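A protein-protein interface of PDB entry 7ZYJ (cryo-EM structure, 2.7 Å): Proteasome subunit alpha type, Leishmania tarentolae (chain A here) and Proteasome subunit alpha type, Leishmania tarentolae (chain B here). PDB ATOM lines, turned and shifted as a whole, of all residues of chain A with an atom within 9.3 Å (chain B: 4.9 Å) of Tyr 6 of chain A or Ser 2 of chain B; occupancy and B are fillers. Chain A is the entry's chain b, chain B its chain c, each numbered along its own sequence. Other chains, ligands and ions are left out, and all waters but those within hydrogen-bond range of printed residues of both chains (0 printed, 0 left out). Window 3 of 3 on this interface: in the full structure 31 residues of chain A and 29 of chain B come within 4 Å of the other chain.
The backbone carbonyl oxygen (O) of Ser 2 of chain B is in hydrogen-bond range of the side-chain hydroxyl (OH) of Tyr 6 of chain A, at 2.6 Å.
The backbone NH (N) of Gly 7 of chain A lies within hydrogen-bond range of the backbone carbonyl oxygen (O) of Gly 132 of chain B, at 3.1 Å.
Tyr 5 of chain B touches Tyr 6 of chain A (O to CE1, 3.7 Å).
Tyr 6 of chain A touches Asp 6 of chain B (CB to OD1, 3.2 Å).
CA of Tyr 6 of chain A touches O of Gly 132 of chain B, at 3.6 Å.
Gly 7 of chain A touches Ser 7 of chain B.
Thr 10 of chain A touches Ser 7 of chain B.
CB of Val 133 of chain B touches O of Gln 121 of chain A, 3.5 Å away.
N of Gly 123 of chain A touches CG1 of Val 133 of chain B, at 3.6 Å.
Hydrophobic or aromatic side chains of chain B that line the printed part of chain A: Tyr 5 and Val 133.
Printed residues of chain A that touch a printed residue of chain B: Tyr 6, Gly 7, Thr 10, Gln 121 and Gly 123.
Hydrophobic or aromatic side chains of chain A within 4 Å of the printed part of chain B: Tyr 6.
Among the printed residues, no Asp or Glu carboxylate lies within 4 Å of a Lys or Arg side-chain nitrogen of the other chain.
O of Tyr 6 of chain A is in hydrogen-bond range of N of Gly 124 of chain A (2.6 Å).
Of the printed residues of chain B, Tyr 6 of chain A touches Ser 2, Tyr 5, Asp 6 and Gly 132.
Thr 9 of chain A touches none of the printed residues of chain B.
Printed residues of chain B within 4 Å of Gln 121 of chain A: Val 133.
Of the printed residues of chain B, Gly 123 of chain A touches Val 133 (3.6 Å).
Arg 126 of chain A touches none of the printed residues of chain B.
Ser 2 of chain B touches just one residue of chain A: Tyr 6 (2.6 Å).
Tyr 5 of chain B touches one residue of chain A.
The nearest printed residue of chain B that does not touch Tyr 6 of chain A is Val 133 of chain B (4.7 Å).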
ATOM      1  N   GLU A   3     -25.677  15.834   2.813  1.00  0.00           N
ATOM      2  CA  GLU A   3     -24.664  16.586   2.081  1.00  0.00           C
ATOM      3  C   GLU A   3     -25.142  17.997   1.768  1.00  0.00           C
ATOM      4  O   GLU A   3     -25.414  18.326   0.613  1.00  0.00           O
ATOM      5  CB  GLU A   3     -24.283  15.858   0.789  1.00  0.00           C
ATOM      6  CG  GLU A   3     -23.377  14.654   1.001  1.00  0.00           C
ATOM      7  CD  GLU A   3     -24.132  13.423   1.464  1.00  0.00           C
ATOM      8  OE1 GLU A   3     -25.380  13.464   1.505  1.00  0.00           O
ATOM      9  OE2 GLU A   3     -23.473  12.413   1.790  1.00  0.00           O
ATOM     10  N   ALA A   4     -25.234  18.823   2.812  1.00  0.00           N
ATOM     11  CA  ALA A   4     -25.661  20.218   2.707  1.00  0.00           C
ATOM     12  C   ALA A   4     -27.050  20.317   2.068  1.00  0.00           C
ATOM     13  O   ALA A   4     -27.240  20.869   0.984  1.00  0.00           O
ATOM     14  CB  ALA A   4     -24.630  21.050   1.933  1.00  0.00           C
ATOM     15  N   PHE A   5     -28.019  19.738   2.774  1.00  0.00           N
ATOM     16  CA  PHE A   5     -29.416  19.809   2.375  1.00  0.00           C
ATOM     17  C   PHE A   5     -30.231  20.768   3.231  1.00  0.00           C
ATOM     18  O   PHE A   5     -31.426  20.941   2.974  1.00  0.00           O
ATOM     19  CB  PHE A   5     -30.052  18.417   2.413  1.00  0.00           C
ATOM     20  CG  PHE A   5     -29.615  17.522   1.290  1.00  0.00           C
ATOM     21  CD1 PHE A   5     -30.084  17.726   0.004  1.00  0.00           C
ATOM     22  CD2 PHE A   5     -28.738  16.477   1.520  1.00  0.00           C
ATOM     23  CE1 PHE A   5     -29.685  16.907  -1.032  1.00  0.00           C
ATOM     24  CE2 PHE A   5     -28.335  15.653   0.487  1.00  0.00           C
ATOM     25  CZ  PHE A   5     -28.809  15.869  -0.790  1.00  0.00           C
ATOM     26  N   TYR A   6     -29.624  21.393   4.233  1.00  0.00           N
ATOM     27  CA  TYR A   6     -30.320  22.381   5.038  1.00  0.00           C
ATOM     28  C   TYR A   6     -30.157  23.770   4.429  1.00  0.00           C
ATOM     29  O   TYR A   6     -29.214  24.042   3.681  1.00  0.00           O
ATOM     30  CB  TYR A   6     -29.816  22.366   6.483  1.00  0.00           C
ATOM     31  CG  TYR A   6     -28.322  22.551   6.645  1.00  0.00           C
ATOM     32  CD1 TYR A   6     -27.751  23.817   6.623  1.00  0.00           C
ATOM     33  CD2 TYR A   6     -27.486  21.460   6.831  1.00  0.00           C
ATOM     34  CE1 TYR A   6     -26.390  23.988   6.776  1.00  0.00           C
ATOM     35  CE2 TYR A   6     -26.125  21.621   6.984  1.00  0.00           C
ATOM     36  CZ  TYR A   6     -25.582  22.887   6.956  1.00  0.00           C
ATOM     37  OH  TYR A   6     -24.226  23.053   7.108  1.00  0.00           O
ATOM     38  N   GLY A   7     -31.094  24.654   4.761  1.00  0.00           N
ATOM     39  CA  GLY A   7     -31.092  25.986   4.185  1.00  0.00           C
ATOM     40  C   GLY A   7     -30.073  26.893   4.857  1.00  0.00           C
ATOM     41  O   GLY A   7     -29.856  26.834   6.067  1.00  0.00           O
ATOM     42  N   LEU A   8     -29.446  27.743   4.047  1.00  0.00           N
ATOM     43  CA  LEU A   8     -28.493  28.719   4.558  1.00  0.00           C
ATOM     44  C   LEU A   8     -29.128  30.080   4.792  1.00  0.00           C
ATOM     45  O   LEU A   8     -28.622  30.860   5.607  1.00  0.00           O
ATOM     46  CB  LEU A   8     -27.313  28.860   3.593  1.00  0.00           C
ATOM     47  CG  LEU A   8     -26.588  27.565   3.220  1.00  0.00           C
ATOM     48  CD1 LEU A   8     -25.347  27.863   2.394  1.00  0.00           C
ATOM     49  CD2 LEU A   8     -26.226  26.774   4.464  1.00  0.00           C
ATOM     50  N   THR A   9     -30.222  30.381   4.099  1.00  0.00           N
ATOM     51  CA  THR A   9     -30.969  31.612   4.315  1.00  0.00           C
ATOM     52  C   THR A   9     -32.142  31.319   5.241  1.00  0.00           C
ATOM     53  O   THR A   9     -33.000  30.489   4.922  1.00  0.00           O
ATOM     54  CB  THR A   9     -31.463  32.190   2.990  1.00  0.00           C
ATOM     55  OG1 THR A   9     -30.348  32.428   2.124  1.00  0.00           O
ATOM     56  CG2 THR A   9     -32.206  33.497   3.223  1.00  0.00           C
ATOM     57  N   THR A  10     -32.175  31.992   6.389  1.00  0.00           N
ATOM     58  CA  THR A  10     -33.248  31.823   7.357  1.00  0.00           C
ATOM     59  C   THR A  10     -33.707  33.191   7.838  1.00  0.00           C
ATOM     60  O   THR A  10     -32.991  34.186   7.724  1.00  0.00           O
ATOM     61  CB  THR A  10     -32.818  30.970   8.560  1.00  0.00           C
ATOM     62  OG1 THR A  10     -31.792  31.652   9.292  1.00  0.00           O
ATOM     63  CG2 THR A  10     -32.302  29.613   8.109  1.00  0.00           C
ATOM     64  N   PHE A 119     -32.394  29.912  -5.216  1.00  0.00           N
ATOM     65  CA  PHE A 119     -31.148  29.919  -4.461  1.00  0.00           C
ATOM     66  C   PHE A 119     -31.247  30.702  -3.159  1.00  0.00           C
ATOM     67  O   PHE A 119     -30.374  30.550  -2.297  1.00  0.00           O
ATOM     68  CB  PHE A 119     -30.012  30.469  -5.322  1.00  0.00           C
ATOM     69  CG  PHE A 119     -29.383  29.438  -6.211  1.00  0.00           C
ATOM     70  CD1 PHE A 119     -30.036  28.994  -7.347  1.00  0.00           C
ATOM     71  CD2 PHE A 119     -28.148  28.897  -5.900  1.00  0.00           C
ATOM     72  CE1 PHE A 119     -29.462  28.041  -8.162  1.00  0.00           C
ATOM     73  CE2 PHE A 119     -27.569  27.943  -6.712  1.00  0.00           C
ATOM     74  CZ  PHE A 119     -28.227  27.514  -7.844  1.00  0.00           C
ATOM     75  N   GLN A 121     -33.915  30.241  -1.201  1.00  0.00           N
ATOM     76  CA  GLN A 121     -34.724  29.418  -0.310  1.00  0.00           C
ATOM     77  C   GLN A 121     -34.315  27.952  -0.247  1.00  0.00           C
ATOM     78  O   GLN A 121     -34.468  27.343   0.819  1.00  0.00           O
ATOM     79  CB  GLN A 121     -36.209  29.503  -0.700  1.00  0.00           C
ATOM     80  CG  GLN A 121     -37.131  28.748   0.240  1.00  0.00           C
ATOM     81  CD  GLN A 121     -38.590  28.893  -0.123  1.00  0.00           C
ATOM     82  OE1 GLN A 121     -38.935  29.534  -1.114  1.00  0.00           O
ATOM     83  NE2 GLN A 121     -39.459  28.321   0.695  1.00  0.00           N
ATOM     84  N   SER A 122     -33.782  27.370  -1.318  1.00  0.00           N
ATOM     85  CA  SER A 122     -33.433  25.957  -1.292  1.00  0.00           C
ATOM     86  C   SER A 122     -32.225  25.725  -0.384  1.00  0.00           C
ATOM     87  O   SER A 122     -31.492  26.649  -0.021  1.00  0.00           O
ATOM     88  CB  SER A 122     -33.166  25.446  -2.706  1.00  0.00           C
ATOM     89  OG  SER A 122     -32.088  26.142  -3.301  1.00  0.00           O
ATOM     90  N   GLY A 123     -32.018  24.463  -0.014  1.00  0.00           N
ATOM     91  CA  GLY A 123     -31.026  24.114   0.984  1.00  0.00           C
ATOM     92  C   GLY A 123     -29.642  23.922   0.399  1.00  0.00           C
ATOM     93  O   GLY A 123     -29.493  23.464  -0.737  1.00  0.00           O
ATOM     94  N   GLY A 124     -28.628  24.279   1.184  1.00  0.00           N
ATOM     95  CA  GLY A 124     -27.248  24.041   0.817  1.00  0.00           C
ATOM     96  C   GLY A 124     -26.621  25.068  -0.095  1.00  0.00           C
ATOM     97  O   GLY A 124     -25.456  24.905  -0.471  1.00  0.00           O
ATOM     98  N   VAL A 125     -27.343  26.127  -0.460  1.00  0.00           N
ATOM     99  CA  VAL A 125     -26.826  27.130  -1.379  1.00  0.00           C
ATOM    100  C   VAL A 125     -27.038  28.513  -0.783  1.00  0.00           C
ATOM    101  O   VAL A 125     -27.872  28.719   0.100  1.00  0.00           O
ATOM    102  CB  VAL A 125     -27.484  27.042  -2.774  1.00  0.00           C
ATOM    103  CG1 VAL A 125     -27.070  25.760  -3.477  1.00  0.00           C
ATOM    104  CG2 VAL A 125     -28.995  27.131  -2.655  1.00  0.00           C
ATOM    105  N   ARG A 126     -26.259  29.463  -1.281  1.00  0.00           N
ATOM    106  CA  ARG A 126     -26.344  30.861  -0.903  1.00  0.00           C
ATOM    107  C   ARG A 126     -26.952  31.677  -2.036  1.00  0.00           C
ATOM    108  O   ARG A 126     -26.927  31.258  -3.199  1.00  0.00           O
ATOM    109  CB  ARG A 126     -24.953  31.411  -0.556  1.00  0.00           C
ATOM    110  CG  ARG A 126     -23.935  31.268  -1.671  1.00  0.00           C
ATOM    111  CD  ARG A 126     -22.862  32.337  -1.577  1.00  0.00           C
ATOM    112  NE  ARG A 126     -21.887  32.219  -2.653  1.00  0.00           N
ATOM    113  CZ  ARG A 126     -22.032  32.752  -3.859  1.00  0.00           C
ATOM    114  NH1 ARG A 126     -23.108  33.451  -4.179  1.00  0.00           N
ATOM    115  NH2 ARG A 126     -21.076  32.577  -4.765  1.00  0.00           N
ATOM    116  N   SER B   2     -21.592  20.942   7.007  1.00  0.00           N
ATOM    117  CA  SER B   2     -21.594  20.094   8.194  1.00  0.00           C
ATOM    118  C   SER B   2     -22.798  20.391   9.080  1.00  0.00           C
ATOM    119  O   SER B   2     -23.428  21.442   8.957  1.00  0.00           O
ATOM    120  CB  SER B   2     -20.300  20.277   8.986  1.00  0.00           C
ATOM    121  OG  SER B   2     -20.231  21.568   9.561  1.00  0.00           O
ATOM    122  N   HIS B   3     -23.110  19.457   9.981  1.00  0.00           N
ATOM    123  CA  HIS B   3     -24.273  19.604  10.847  1.00  0.00           C
ATOM    124  C   HIS B   3     -24.101  20.711  11.878  1.00  0.00           C
ATOM    125  O   HIS B   3     -25.090  21.125  12.491  1.00  0.00           O
ATOM    126  CB  HIS B   3     -24.572  18.279  11.550  1.00  0.00           C
ATOM    127  CG  HIS B   3     -23.619  17.953  12.657  1.00  0.00           C
ATOM    128  ND1 HIS B   3     -23.809  18.381  13.954  1.00  0.00           N
ATOM    129  CD2 HIS B   3     -22.467  17.242  12.662  1.00  0.00           C
ATOM    130  CE1 HIS B   3     -22.816  17.946  14.708  1.00  0.00           C
ATOM    131  NE2 HIS B   3     -21.988  17.252  13.949  1.00  0.00           N
ATOM    132  N   ARG B   4     -22.875  21.197  12.087  1.00  0.00           N
ATOM    133  CA  ARG B   4     -22.652  22.283  13.033  1.00  0.00           C
ATOM    134  C   ARG B   4     -23.374  23.561  12.630  1.00  0.00           C
ATOM    135  O   ARG B   4     -23.895  24.266  13.501  1.00  0.00           O
ATOM    136  CB  ARG B   4     -21.158  22.574  13.169  1.00  0.00           C
ATOM    137  CG  ARG B   4     -20.326  21.413  13.677  1.00  0.00           C
ATOM    138  CD  ARG B   4     -18.914  21.873  13.997  1.00  0.00           C
ATOM    139  NE  ARG B   4     -18.875  22.696  15.200  1.00  0.00           N
ATOM    140  CZ  ARG B   4     -17.821  23.396  15.597  1.00  0.00           C
ATOM    141  NH1 ARG B   4     -16.697  23.407  14.902  1.00  0.00           N
ATOM    142  NH2 ARG B   4     -17.900  24.105  16.719  1.00  0.00           N
ATOM    143  N   TYR B   5     -23.417  23.872  11.337  1.00  0.00           N
ATOM    144  CA  TYR B   5     -23.979  25.119  10.844  1.00  0.00           C
ATOM    145  C   TYR B   5     -25.445  24.991  10.452  1.00  0.00           C
ATOM    146  O   TYR B   5     -26.018  25.944   9.917  1.00  0.00           O
ATOM    147  CB  TYR B   5     -23.152  25.623   9.661  1.00  0.00           C
ATOM    148  CG  TYR B   5     -21.662  25.523   9.902  1.00  0.00           C
ATOM    149  CD1 TYR B   5     -21.061  26.216  10.943  1.00  0.00           C
ATOM    150  CD2 TYR B   5     -20.863  24.721   9.102  1.00  0.00           C
ATOM    151  CE1 TYR B   5     -19.703  26.125  11.173  1.00  0.00           C
ATOM    152  CE2 TYR B   5     -19.503  24.623   9.324  1.00  0.00           C
ATOM    153  CZ  TYR B   5     -18.929  25.327  10.360  1.00  0.00           C
ATOM    154  OH  TYR B   5     -17.576  25.231  10.586  1.00  0.00           O
ATOM    155  N   ASP B   6     -26.060  23.837  10.699  1.00  0.00           N
ATOM    156  CA  ASP B   6     -27.480  23.661  10.428  1.00  0.00           C
ATOM    157  C   ASP B   6     -28.293  24.523  11.388  1.00  0.00           C
ATOM    158  O   ASP B   6     -28.102  24.457  12.606  1.00  0.00           O
ATOM    159  CB  ASP B   6     -27.862  22.189  10.565  1.00  0.00           C
ATOM    160  CG  ASP B   6     -29.281  21.906  10.111  1.00  0.00           C
ATOM    161  OD1 ASP B   6     -29.969  22.843   9.656  1.00  0.00           O
ATOM    162  OD2 ASP B   6     -29.712  20.738  10.207  1.00  0.00           O
ATOM    163  N   SER B   7     -29.199  25.331  10.837  1.00  0.00           N
ATOM    164  CA  SER B   7     -30.000  26.234  11.653  1.00  0.00           C
ATOM    165  C   SER B   7     -31.209  25.554  12.281  1.00  0.00           C
ATOM    166  O   SER B   7     -31.803  26.117  13.206  1.00  0.00           O
ATOM    167  CB  SER B   7     -30.462  27.426  10.815  1.00  0.00           C
ATOM    168  OG  SER B   7     -31.316  27.005   9.769  1.00  0.00           O
ATOM    169  N   GLY B 132     -36.070  20.992   5.986  1.00  0.00           N
ATOM    170  CA  GLY B 132     -34.968  21.669   6.638  1.00  0.00           C
ATOM    171  C   GLY B 132     -34.615  23.014   6.050  1.00  0.00           C
ATOM    172  O   GLY B 132     -33.506  23.505   6.273  1.00  0.00           O
ATOM    173  N   VAL B 133     -35.529  23.630   5.302  1.00  0.00           N
ATOM    174  CA  VAL B 133     -35.296  24.944   4.716  1.00  0.00           C
ATOM    175  C   VAL B 133     -36.273  25.936   5.329  1.00  0.00           C
ATOM    176  O   VAL B 133     -37.169  25.554   6.089  1.00  0.00           O
ATOM    177  CB  VAL B 133     -35.432  24.907   3.182  1.00  0.00           C
ATOM    178  CG1 VAL B 133     -34.468  23.895   2.588  1.00  0.00           C
ATOM    179  CG2 VAL B 133     -36.862  24.585   2.785  1.00  0.00           C
